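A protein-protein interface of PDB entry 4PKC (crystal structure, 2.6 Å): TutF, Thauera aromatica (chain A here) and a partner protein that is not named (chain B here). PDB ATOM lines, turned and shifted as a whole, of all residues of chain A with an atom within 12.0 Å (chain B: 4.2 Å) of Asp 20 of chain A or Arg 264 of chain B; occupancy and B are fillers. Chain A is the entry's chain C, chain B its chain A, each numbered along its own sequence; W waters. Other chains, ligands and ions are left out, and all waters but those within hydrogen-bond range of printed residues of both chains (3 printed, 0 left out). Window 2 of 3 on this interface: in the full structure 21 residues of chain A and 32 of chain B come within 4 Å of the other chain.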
ATOM      1  N   PHE A  13       4.831  14.151 -15.063  1.00  0.00           N
ATOM      2  CA  PHE A  13       4.030  15.351 -15.285  1.00  0.00           C
ATOM      3  C   PHE A  13       4.924  16.546 -15.602  1.00  0.00           C
ATOM      4  O   PHE A  13       5.551  17.110 -14.705  1.00  0.00           O
ATOM      5  CB  PHE A  13       3.156  15.656 -14.066  1.00  0.00           C
ATOM      6  CG  PHE A  13       2.060  14.652 -13.839  1.00  0.00           C
ATOM      7  CD1 PHE A  13       0.833  14.794 -14.467  1.00  0.00           C
ATOM      8  CD2 PHE A  13       2.255  13.571 -12.996  1.00  0.00           C
ATOM      9  CE1 PHE A  13      -0.177  13.874 -14.259  1.00  0.00           C
ATOM     10  CE2 PHE A  13       1.249  12.649 -12.784  1.00  0.00           C
ATOM     11  CZ  PHE A  13       0.031  12.800 -13.415  1.00  0.00           C
ATOM     12  N   PRO A  14       4.983  16.930 -16.888  1.00  0.00           N
ATOM     13  CA  PRO A  14       5.809  18.044 -17.368  1.00  0.00           C
ATOM     14  C   PRO A  14       5.544  19.343 -16.615  1.00  0.00           C
ATOM     15  O   PRO A  14       4.390  19.746 -16.463  1.00  0.00           O
ATOM     16  CB  PRO A  14       5.396  18.179 -18.837  1.00  0.00           C
ATOM     17  CG  PRO A  14       4.924  16.824 -19.216  1.00  0.00           C
ATOM     18  CD  PRO A  14       4.259  16.270 -17.989  1.00  0.00           C
ATOM     19  N   VAL A  15       6.608  19.984 -16.147  1.00  0.00           N
ATOM     20  CA  VAL A  15       6.487  21.256 -15.448  1.00  0.00           C
ATOM     21  C   VAL A  15       6.116  22.361 -16.430  1.00  0.00           C
ATOM     22  O   VAL A  15       6.783  22.535 -17.450  1.00  0.00           O
ATOM     23  CB  VAL A  15       7.794  21.624 -14.719  1.00  0.00           C
ATOM     24  CG1 VAL A  15       7.685  23.004 -14.090  1.00  0.00           C
ATOM     25  CG2 VAL A  15       8.127  20.575 -13.668  1.00  0.00           C
ATOM     26  N   PRO A  16       5.036  23.101 -16.129  1.00  0.00           N
ATOM     27  CA  PRO A  16       4.566  24.220 -16.955  1.00  0.00           C
ATOM     28  C   PRO A  16       5.660  25.247 -17.229  1.00  0.00           C
ATOM     29  O   PRO A  16       6.529  25.465 -16.385  1.00  0.00           O
ATOM     30  CB  PRO A  16       3.444  24.828 -16.109  1.00  0.00           C
ATOM     31  CG  PRO A  16       2.938  23.688 -15.299  1.00  0.00           C
ATOM     32  CD  PRO A  16       4.145  22.851 -14.982  1.00  0.00           C
ATOM     33  N   LYS A  17       5.608  25.873 -18.401  1.00  0.00           N
ATOM     34  CA  LYS A  17       6.652  26.796 -18.833  1.00  0.00           C
ATOM     35  C   LYS A  17       6.632  28.114 -18.061  1.00  0.00           C
ATOM     36  O   LYS A  17       7.571  28.904 -18.148  1.00  0.00           O
ATOM     37  CB  LYS A  17       6.521  27.073 -20.332  1.00  0.00           C
ATOM     38  CG  LYS A  17       6.625  25.827 -21.199  1.00  0.00           C
ATOM     39  CD  LYS A  17       6.339  26.138 -22.661  1.00  0.00           C
ATOM     40  CE  LYS A  17       7.346  27.123 -23.230  1.00  0.00           C
ATOM     41  NZ  LYS A  17       7.072  27.423 -24.663  1.00  0.00           N
ATOM     42  N   ASP A  18       5.563  28.348 -17.306  1.00  0.00           N
ATOM     43  CA  ASP A  18       5.428  29.591 -16.553  1.00  0.00           C
ATOM     44  C   ASP A  18       5.722  29.389 -15.070  1.00  0.00           C
ATOM     45  O   ASP A  18       5.628  30.325 -14.278  1.00  0.00           O
ATOM     46  CB  ASP A  18       4.025  30.176 -16.733  1.00  0.00           C
ATOM     47  CG  ASP A  18       2.943  29.291 -16.149  1.00  0.00           C
ATOM     48  OD1 ASP A  18       3.180  28.073 -16.008  1.00  0.00           O
ATOM     49  OD2 ASP A  18       1.855  29.814 -15.830  1.00  0.00           O
ATOM     50  N   ALA A  19       6.080  28.164 -14.698  1.00  0.00           N
ATOM     51  CA  ALA A  19       6.392  27.852 -13.308  1.00  0.00           C
ATOM     52  C   ALA A  19       7.727  28.464 -12.894  1.00  0.00           C
ATOM     53  O   ALA A  19       8.630  28.618 -13.716  1.00  0.00           O
ATOM     54  CB  ALA A  19       6.410  26.347 -13.094  1.00  0.00           C
ATOM     55  N   ASP A  20       7.839  28.808 -11.614  1.00  0.00           N
ATOM     56  CA  ASP A  20       9.059  29.399 -11.074  1.00  0.00           C
ATOM     57  C   ASP A  20      10.247  28.452 -11.203  1.00  0.00           C
ATOM     58  O   ASP A  20      11.387  28.888 -11.367  1.00  0.00           O
ATOM     59  CB  ASP A  20       8.864  29.782  -9.603  1.00  0.00           C
ATOM     60  CG  ASP A  20       7.803  30.849  -9.411  1.00  0.00           C
ATOM     61  OD1 ASP A  20       7.566  31.634 -10.352  1.00  0.00           O
ATOM     62  OD2 ASP A  20       7.209  30.908  -8.313  1.00  0.00           O
ATOM     63  N   ASP A  21       9.973  27.155 -11.130  1.00  0.00           N
ATOM     64  CA  ASP A  21      11.023  26.145 -11.158  1.00  0.00           C
ATOM     65  C   ASP A  21      11.151  25.488 -12.527  1.00  0.00           C
ATOM     66  O   ASP A  21      11.751  24.422 -12.650  1.00  0.00           O
ATOM     67  CB  ASP A  21      10.753  25.072 -10.103  1.00  0.00           C
ATOM     68  CG  ASP A  21       9.461  24.321 -10.355  1.00  0.00           C
ATOM     69  OD1 ASP A  21       8.493  24.945 -10.839  1.00  0.00           O
ATOM     70  OD2 ASP A  21       9.412  23.104 -10.075  1.00  0.00           O
ATOM     71  N   TYR A  22      10.589  26.120 -13.552  1.00  0.00           N
ATOM     72  CA  TYR A  22      10.585  25.520 -14.882  1.00  0.00           C
ATOM     73  C   TYR A  22      11.974  25.449 -15.500  1.00  0.00           C
ATOM     74  O   TYR A  22      12.694  26.445 -15.563  1.00  0.00           O
ATOM     75  CB  TYR A  22       9.656  26.284 -15.826  1.00  0.00           C
ATOM     76  CG  TYR A  22       9.773  25.814 -17.259  1.00  0.00           C
ATOM     77  CD1 TYR A  22       9.248  24.589 -17.652  1.00  0.00           C
ATOM     78  CD2 TYR A  22      10.422  26.585 -18.216  1.00  0.00           C
ATOM     79  CE1 TYR A  22       9.357  24.149 -18.957  1.00  0.00           C
ATOM     80  CE2 TYR A  22      10.537  26.152 -19.525  1.00  0.00           C
ATOM     81  CZ  TYR A  22      10.003  24.933 -19.889  1.00  0.00           C
ATOM     82  OH  TYR A  22      10.111  24.496 -21.190  1.00  0.00           O
ATOM     83  N   GLU A  23      12.337  24.258 -15.960  1.00  0.00           N
ATOM     84  CA  GLU A  23      13.569  24.054 -16.709  1.00  0.00           C
ATOM     85  C   GLU A  23      13.292  23.121 -17.883  1.00  0.00           C
ATOM     86  O   GLU A  23      12.264  22.442 -17.914  1.00  0.00           O
ATOM     87  CB  GLU A  23      14.670  23.489 -15.808  1.00  0.00           C
ATOM     88  CG  GLU A  23      15.227  24.497 -14.811  1.00  0.00           C
ATOM     89  CD  GLU A  23      16.284  23.906 -13.899  1.00  0.00           C
ATOM     90  OE1 GLU A  23      17.342  24.545 -13.720  1.00  0.00           O
ATOM     91  OE2 GLU A  23      16.054  22.807 -13.352  1.00  0.00           O
ATOM     92  N   ALA A  24      14.203  23.099 -18.849  1.00  0.00           N
ATOM     93  CA  ALA A  24      14.024  22.296 -20.054  1.00  0.00           C
ATOM     94  C   ALA A  24      13.939  20.806 -19.733  1.00  0.00           C
ATOM     95  O   ALA A  24      14.818  20.251 -19.074  1.00  0.00           O
ATOM     96  CB  ALA A  24      15.156  22.561 -21.036  1.00  0.00           C
ATOM     97  N   LYS A  26      12.047  19.299 -17.742  1.00  0.00           N
ATOM     98  CA  LYS A  26      11.776  19.032 -16.335  1.00  0.00           C
ATOM     99  C   LYS A  26      10.346  18.538 -16.146  1.00  0.00           C
ATOM    100  O   LYS A  26       9.434  18.962 -16.858  1.00  0.00           O
ATOM    101  CB  LYS A  26      12.022  20.289 -15.497  1.00  0.00           C
ATOM    102  CG  LYS A  26      11.989  20.057 -13.995  1.00  0.00           C
ATOM    103  CD  LYS A  26      12.171  21.361 -13.238  1.00  0.00           C
ATOM    104  CE  LYS A  26      12.189  21.133 -11.736  1.00  0.00           C
ATOM    105  NZ  LYS A  26      13.337  20.283 -11.319  1.00  0.00           N
ATOM    106  N   ALA A  27      10.152  17.640 -15.187  1.00  0.00           N
ATOM    107  CA  ALA A  27       8.831  17.077 -14.937  1.00  0.00           C
ATOM    108  C   ALA A  27       8.683  16.591 -13.499  1.00  0.00           C
ATOM    109  O   ALA A  27       9.671  16.319 -12.818  1.00  0.00           O
ATOM    110  CB  ALA A  27       8.555  15.940 -15.906  1.00  0.00           C
ATOM    111  N   ASP A  28       7.438  16.489 -13.046  1.00  0.00           N
ATOM    112  CA  ASP A  28       7.146  15.945 -11.726  1.00  0.00           C
ATOM    113  C   ASP A  28       6.824  14.460 -11.830  1.00  0.00           C
ATOM    114  O   ASP A  28       5.906  14.067 -12.551  1.00  0.00           O
ATOM    115  CB  ASP A  28       5.974  16.688 -11.073  1.00  0.00           C
ATOM    116  CG  ASP A  28       6.295  18.138 -10.762  1.00  0.00           C
ATOM    117  OD1 ASP A  28       7.474  18.447 -10.489  1.00  0.00           O
ATOM    118  OD2 ASP A  28       5.360  18.969 -10.782  1.00  0.00           O
ATOM    119  N   VAL A  30       5.064  11.936 -10.146  1.00  0.00           N
ATOM    120  CA  VAL A  30       4.079  11.701  -9.100  1.00  0.00           C
ATOM    121  C   VAL A  30       3.736  10.221  -8.981  1.00  0.00           C
ATOM    122  O   VAL A  30       3.258   9.607  -9.932  1.00  0.00           O
ATOM    123  CB  VAL A  30       2.788  12.499  -9.352  1.00  0.00           C
ATOM    124  CG1 VAL A  30       1.794  12.261  -8.225  1.00  0.00           C
ATOM    125  CG2 VAL A  30       3.101  13.981  -9.489  1.00  0.00           C
ATOM    126  N   SER A  43       5.986  13.675  -5.020  1.00  0.00           N
ATOM    127  CA  SER A  43       6.347  14.423  -6.222  1.00  0.00           C
ATOM    128  C   SER A  43       7.849  14.689  -6.287  1.00  0.00           C
ATOM    129  O   SER A  43       8.378  15.504  -5.530  1.00  0.00           O
ATOM    130  CB  SER A  43       5.579  15.745  -6.279  1.00  0.00           C
ATOM    131  OG  SER A  43       5.944  16.500  -7.422  1.00  0.00           O
ATOM    132  N   LYS A  44       8.528  14.003  -7.201  1.00  0.00           N
ATOM    133  CA  LYS A  44       9.973  14.143  -7.350  1.00  0.00           C
ATOM    134  C   LYS A  44      10.343  14.741  -8.704  1.00  0.00           C
ATOM    135  O   LYS A  44       9.924  14.236  -9.745  1.00  0.00           O
ATOM    136  CB  LYS A  44      10.657  12.785  -7.172  1.00  0.00           C
ATOM    137  CG  LYS A  44      12.173  12.838  -7.253  1.00  0.00           C
ATOM    138  CD  LYS A  44      12.781  11.451  -7.119  1.00  0.00           C
ATOM    139  CE  LYS A  44      14.301  11.506  -7.133  1.00  0.00           C
ATOM    140  NZ  LYS A  44      14.840  12.290  -5.985  1.00  0.00           N
ATOM    141  N   PRO A  45      11.126  15.831  -8.691  1.00  0.00           N
ATOM    142  CA  PRO A  45      11.585  16.485  -9.924  1.00  0.00           C
ATOM    143  C   PRO A  45      12.578  15.624 -10.702  1.00  0.00           C
ATOM    144  O   PRO A  45      13.621  15.255 -10.162  1.00  0.00           O
ATOM    145  CB  PRO A  45      12.260  17.766  -9.415  1.00  0.00           C
ATOM    146  CG  PRO A  45      11.750  17.958  -8.025  1.00  0.00           C
ATOM    147  CD  PRO A  45      11.532  16.579  -7.492  1.00  0.00           C
ATOM    148  N   PHE A  47      14.462  14.935 -14.799  1.00  0.00           N
ATOM    149  CA  PHE A  47      14.783  15.551 -16.085  1.00  0.00           C
ATOM    150  C   PHE A  47      14.799  14.558 -17.250  1.00  0.00           C
ATOM    151  O   PHE A  47      15.863  14.071 -17.635  1.00  0.00           O
ATOM    152  CB  PHE A  47      16.140  16.258 -16.007  1.00  0.00           C
ATOM    153  CG  PHE A  47      16.091  17.595 -15.326  1.00  0.00           C
ATOM    154  CD1 PHE A  47      16.271  17.699 -13.956  1.00  0.00           C
ATOM    155  CD2 PHE A  47      15.868  18.749 -16.059  1.00  0.00           C
ATOM    156  CE1 PHE A  47      16.225  18.933 -13.329  1.00  0.00           C
ATOM    157  CE2 PHE A  47      15.820  19.984 -15.438  1.00  0.00           C
ATOM    158  CZ  PHE A  47      15.999  20.074 -14.072  1.00  0.00           C
ATOM    159  N   ILE B 260       9.305  30.092  -2.097  1.00  0.00           N
ATOM    160  CA  ILE B 260       8.133  30.365  -2.924  1.00  0.00           C
ATOM    161  C   ILE B 260       7.934  29.265  -3.961  1.00  0.00           C
ATOM    162  O   ILE B 260       6.835  28.727  -4.108  1.00  0.00           O
ATOM    163  CB  ILE B 260       8.251  31.721  -3.644  1.00  0.00           C
ATOM    164  CG1 ILE B 260       8.171  32.870  -2.639  1.00  0.00           C
ATOM    165  CG2 ILE B 260       7.159  31.869  -4.689  1.00  0.00           C
ATOM    166  CD1 ILE B 260       8.241  34.237  -3.279  1.00  0.00           C
ATOM    167  N   SER B 261       9.009  28.934  -4.670  1.00  0.00           N
ATOM    168  CA  SER B 261       8.988  27.874  -5.672  1.00  0.00           C
ATOM    169  C   SER B 261       8.651  26.523  -5.044  1.00  0.00           C
ATOM    170  O   SER B 261       7.924  25.719  -5.625  1.00  0.00           O
ATOM    171  CB  SER B 261      10.339  27.802  -6.388  1.00  0.00           C
ATOM    172  OG  SER B 261      10.390  26.707  -7.285  1.00  0.00           O
ATOM    173  N   TRP B 262       9.186  26.291  -3.851  1.00  0.00           N
ATOM    174  CA  TRP B 262       8.957  25.057  -3.107  1.00  0.00           C
ATOM    175  C   TRP B 262       7.502  24.933  -2.662  1.00  0.00           C
ATOM    176  O   TRP B 262       6.921  23.848  -2.695  1.00  0.00           O
ATOM    177  CB  TRP B 262       9.900  25.006  -1.903  1.00  0.00           C
ATOM    178  CG  TRP B 262       9.609  23.949  -0.888  1.00  0.00           C
ATOM    179  CD1 TRP B 262       9.805  22.608  -1.020  1.00  0.00           C
ATOM    180  CD2 TRP B 262       9.111  24.155   0.440  1.00  0.00           C
ATOM    181  NE1 TRP B 262       9.441  21.962   0.137  1.00  0.00           N
ATOM    182  CE2 TRP B 262       9.013  22.889   1.048  1.00  0.00           C
ATOM    183  CE3 TRP B 262       8.729  25.286   1.169  1.00  0.00           C
ATOM    184  CZ2 TRP B 262       8.549  22.722   2.353  1.00  0.00           C
ATOM    185  CZ3 TRP B 262       8.269  25.118   2.463  1.00  0.00           C
ATOM    186  CH2 TRP B 262       8.183  23.846   3.041  1.00  0.00           C
ATOM    187  N   ALA B 263       6.916  26.053  -2.255  1.00  0.00           N
ATOM    188  CA  ALA B 263       5.524  26.075  -1.822  1.00  0.00           C
ATOM    189  C   ALA B 263       4.577  25.925  -3.008  1.00  0.00           C
ATOM    190  O   ALA B 263       3.523  25.299  -2.897  1.00  0.00           O
ATOM    191  CB  ALA B 263       5.224  27.358  -1.067  1.00  0.00           C
ATOM    192  N   ARG B 264       4.961  26.501  -4.142  1.00  0.00           N
ATOM    193  CA  ARG B 264       4.144  26.433  -5.348  1.00  0.00           C
ATOM    194  C   ARG B 264       4.247  25.068  -6.024  1.00  0.00           C
ATOM    195  O   ARG B 264       3.308  24.620  -6.683  1.00  0.00           O
ATOM    196  CB  ARG B 264       4.544  27.541  -6.322  1.00  0.00           C
ATOM    197  CG  ARG B 264       4.096  28.921  -5.877  1.00  0.00           C
ATOM    198  CD  ARG B 264       4.650  30.015  -6.768  1.00  0.00           C
ATOM    199  NE  ARG B 264       4.055  31.310  -6.453  1.00  0.00           N
ATOM    200  CZ  ARG B 264       4.463  32.466  -6.964  1.00  0.00           C
ATOM    201  NH1 ARG B 264       3.857  33.595  -6.620  1.00  0.00           N
ATOM    202  NH2 ARG B 264       5.480  32.497  -7.816  1.00  0.00           N
ATOM    203  N   ARG B 265       5.387  24.405  -5.855  1.00  0.00           N
ATOM    204  CA  ARG B 265       5.542  23.047  -6.360  1.00  0.00           C
ATOM    205  C   ARG B 265       4.730  22.094  -5.488  1.00  0.00           C
ATOM    206  O   ARG B 265       4.255  21.060  -5.954  1.00  0.00           O
ATOM    207  CB  ARG B 265       7.017  22.636  -6.398  1.00  0.00           C
ATOM    208  CG  ARG B 265       7.262  21.275  -7.038  1.00  0.00           C
ATOM    209  CD  ARG B 265       8.717  21.094  -7.446  1.00  0.00           C
ATOM    210  NE  ARG B 265       9.633  21.225  -6.317  1.00  0.00           N
ATOM    211  CZ  ARG B 265      10.000  20.217  -5.534  1.00  0.00           C
ATOM    212  NH1 ARG B 265      10.840  20.425  -4.529  1.00  0.00           N
ATOM    213  NH2 ARG B 265       9.525  18.999  -5.754  1.00  0.00           N
ATOM    214  N   GLN B 266       4.573  22.460  -4.220  1.00  0.00           N
ATOM    215  CA  GLN B 266       3.720  21.713  -3.303  1.00  0.00           C
ATOM    216  C   GLN B 266       2.264  21.840  -3.731  1.00  0.00           C
ATOM    217  O   GLN B 266       1.496  20.881  -3.658  1.00  0.00           O
ATOM    218  CB  GLN B 266       3.896  22.214  -1.868  1.00  0.00           C
ATOM    219  CG  GLN B 266       2.972  21.551  -0.856  1.00  0.00           C
ATOM    220  CD  GLN B 266       3.431  20.160  -0.466  1.00  0.00           C
ATOM    221  OE1 GLN B 266       4.588  19.958  -0.098  1.00  0.00           O
ATOM    222  NE2 GLN B 266       2.527  19.191  -0.546  1.00  0.00           N
ATOM    223  N   GLY B 267       1.894  23.036  -4.179  1.00  0.00           N
ATOM    224  CA  GLY B 267       0.548  23.292  -4.651  1.00  0.00           C
ATOM    225  C   GLY B 267       0.265  22.578  -5.957  1.00  0.00           C
ATOM    226  O   GLY B 267      -0.850  22.113  -6.192  1.00  0.00           O
ATOM    227  N   ARG B 268       1.284  22.491  -6.806  1.00  0.00           N
ATOM    228  CA  ARG B 268       1.155  21.814  -8.089  1.00  0.00           C
ATOM    229  C   ARG B 268       0.883  20.329  -7.880  1.00  0.00           C
ATOM    230  O   ARG B 268       0.166  19.706  -8.661  1.00  0.00           O
ATOM    231  CB  ARG B 268       2.416  22.019  -8.933  1.00  0.00           C
ATOM    232  CG  ARG B 268       2.300  21.523 -10.364  1.00  0.00           C
ATOM    233  CD  ARG B 268       3.473  21.999 -11.203  1.00  0.00           C
ATOM    234  NE  ARG B 268       4.747  21.487 -10.707  1.00  0.00           N
ATOM    235  CZ  ARG B 268       5.885  22.171 -10.727  1.00  0.00           C
ATOM    236  NH1 ARG B 268       6.998  21.624 -10.255  1.00  0.00           N
ATOM    237  NH2 ARG B 268       5.913  23.404 -11.215  1.00  0.00           N
ATOM    238  N   CYS B 294      -1.386  27.451  -1.661  1.00  0.00           N
ATOM    239  CA  CYS B 294       0.057  27.251  -1.783  1.00  0.00           C
ATOM    240  C   CYS B 294       0.654  28.110  -2.894  1.00  0.00           C
ATOM    241  O   CYS B 294       1.820  28.499  -2.833  1.00  0.00           O
ATOM    242  CB  CYS B 294       0.372  25.776  -2.038  1.00  0.00           C
ATOM    243  SG  CYS B 294      -0.123  24.666  -0.699  1.00  0.00           S
ATOM    244  N   GLN B 295      -0.154  28.406  -3.906  1.00  0.00           N
ATOM    245  CA  GLN B 295       0.284  29.234  -5.021  1.00  0.00           C
ATOM    246  C   GLN B 295       0.533  30.678  -4.586  1.00  0.00           C
ATOM    247  O   GLN B 295       1.533  31.285  -4.969  1.00  0.00           O
ATOM    248  CB  GLN B 295      -0.750  29.197  -6.148  1.00  0.00           C
ATOM    249  CG  GLN B 295      -0.428  30.106  -7.318  1.00  0.00           C
ATOM    250  CD  GLN B 295       0.841  29.703  -8.038  1.00  0.00           C
ATOM    251  OE1 GLN B 295       1.175  28.520  -8.115  1.00  0.00           O
ATOM    252  NE2 GLN B 295       1.560  30.686  -8.567  1.00  0.00           N
ATOM    253  N   ALA B 299       4.096  33.581  -0.982  1.00  0.00           N
ATOM    254  CA  ALA B 299       4.569  34.596  -1.917  1.00  0.00           C
ATOM    255  C   ALA B 299       3.854  35.920  -1.666  1.00  0.00           C
ATOM    256  O   ALA B 299       4.476  36.981  -1.628  1.00  0.00           O
ATOM    257  CB  ALA B 299       4.364  34.141  -3.352  1.00  0.00           C
HETATM  258  O   HOH W   1       4.130  18.933 -12.971  1.00  0.00           O
HETATM  259  O   HOH W   2       6.998  26.492  -8.285  1.00  0.00           O
HETATM  260  O   HOH W   3       8.240  17.565  -7.916  1.00  0.00           O
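NH2 of Arg 264 of chain B lies within salt-bridge range of OD2 of Asp 20 of chain A, at 2.4 Å. The side-chain carboxylate (OD2) of Asp 21 of chain A lies within salt-bridge range of the guanidinium group (NH1) of Arg 268 of chain B (2.8 Å). The side-chain carboxylate (OD2) of Asp 28 of chain A is in salt-bridge range of the guanidinium group (NE) of Arg 268 of chain B, at 2.6 Å.
The backbone carbonyl oxygen of Gln 295 of chain B sits at hydrogen-bond distance from the guanidinium group of Arg 264 of chain B (2.9 Å). The backbone NH (N) of Asp 28 of chain A is in hydrogen-bond range of the backbone carbonyl oxygen (O) of Phe 13 of chain A, 2.6 Å away. The backbone NH (N) of Val 15 of chain A lies within hydrogen-bond range of the backbone carbonyl oxygen (O) of Lys 26 of chain A.
Among the printed residues, pairs that only touch across the chains: Asp 21 of chain A with Ser 261 of chain B (3.3 Å), Pro 45 of chain A with Arg 265 of chain B (3.3 Å), Asp 21 of chain A with Arg 265 of chain B (3.4 Å), Val 15 of chain A with Arg 268 of chain B (3.4 Å), Ala 19 of chain A with Arg 268 of chain B (3.5 Å), Ser 43 of chain A with Arg 265 of chain B (3.7 Å), Asp 20 of chain A with Ile 260 of chain B (3.7 Å) and Pro 16 of chain A with Arg 268 of chain B (3.9 Å).
Phe 13 of chain A touches none of the printed residues of chain B. Of the printed residues of chain B, Val 15 of chain A touches Arg 268. Of the printed residues of chain B, Ala 19 of chain A touches Arg 268. Of the printed residues of chain B, Asp 20 of chain A touches Ile 260 (3.7 Å) and Arg 264 (2.4 Å). Of the printed residues of chain B, Ser 43 of chain A touches Arg 265 (3.7 Å). Lys 44 of chain A touches none of the printed residues of chain B. Ser 261 of chain B touches one residue of chain A. No residue of chain A comes within 4 Å of Ala 263 of chain B. Of chain A, only Asp 20 comes within 4 Å of Arg 264 of chain B. Printed residues of chain A within 4 Å of Arg 265 of chain B: Asp 21 (3.4 Å), Ser 43 (3.7 Å) and Pro 45 (3.3 Å). No residue of chain A comes within 4 Å of Gly 267 of chain B. Arg 268 of chain B touches just these residues of chain A: Val 15, Pro 16, Ala 19, Asp 21 and Asp 28. No residue of chain A comes within 4 Å of Ala 299 of chain B. The nearest residue of chain B that does not touch Asp 20 of chain A is Ser 261 of chain B (4.1 Å). The nearest residue of chain A that does not touch Arg 264 of chain B is Asp 21 of chain A (6.4 Å). The nearest printed residue of chain B that does not touch Asp 28 of chain A is Arg 265 of chain B (4.2 Å).
Of the 12 printed residues of chain B, 5 touch a printed residue of chain A. Printed residues of chain B that touch a printed residue of chain A: Ile 260, Ser 261, Arg 264, Arg 265 and Arg 268. Hydrophobic or aromatic side chains of chain B within 4 Å of the printed part of chain A: Ile 260. Of the 20 printed residues of chain A, 8 touch a printed residue of chain B. Among the printed residues, Asp or Glu carboxylates within 4 Å of a Lys or Arg side-chain nitrogen of the other chain: Asp 20 of chain A with Arg 264 of chain B (2.4 Å), Asp 21 of chain A with Arg 268 of chain B (2.8 Å) and Asp 28 of chain A with Arg 268 of chain B (2.6 Å).
Water W1 lies within hydrogen-bond range of OD2 of Asp 28 of chain A (2.5 Å), O of Phe 13 of chain A (2.9 Å) and NE of Arg 268 of chain B (3.5 Å). Water W3 lies within hydrogen-bond range of the side-chain hydroxyl of Ser 43 of chain A, the side-chain carboxylate of Asp 28 of chain A and the guanidinium group of Arg 265 of chain B. Water W2 bridges the backbone carbonyl oxygen of Ser 261 of chain B (2.9 Å) and the side-chain carboxylate of Asp 21 of chain A (3.3 Å).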
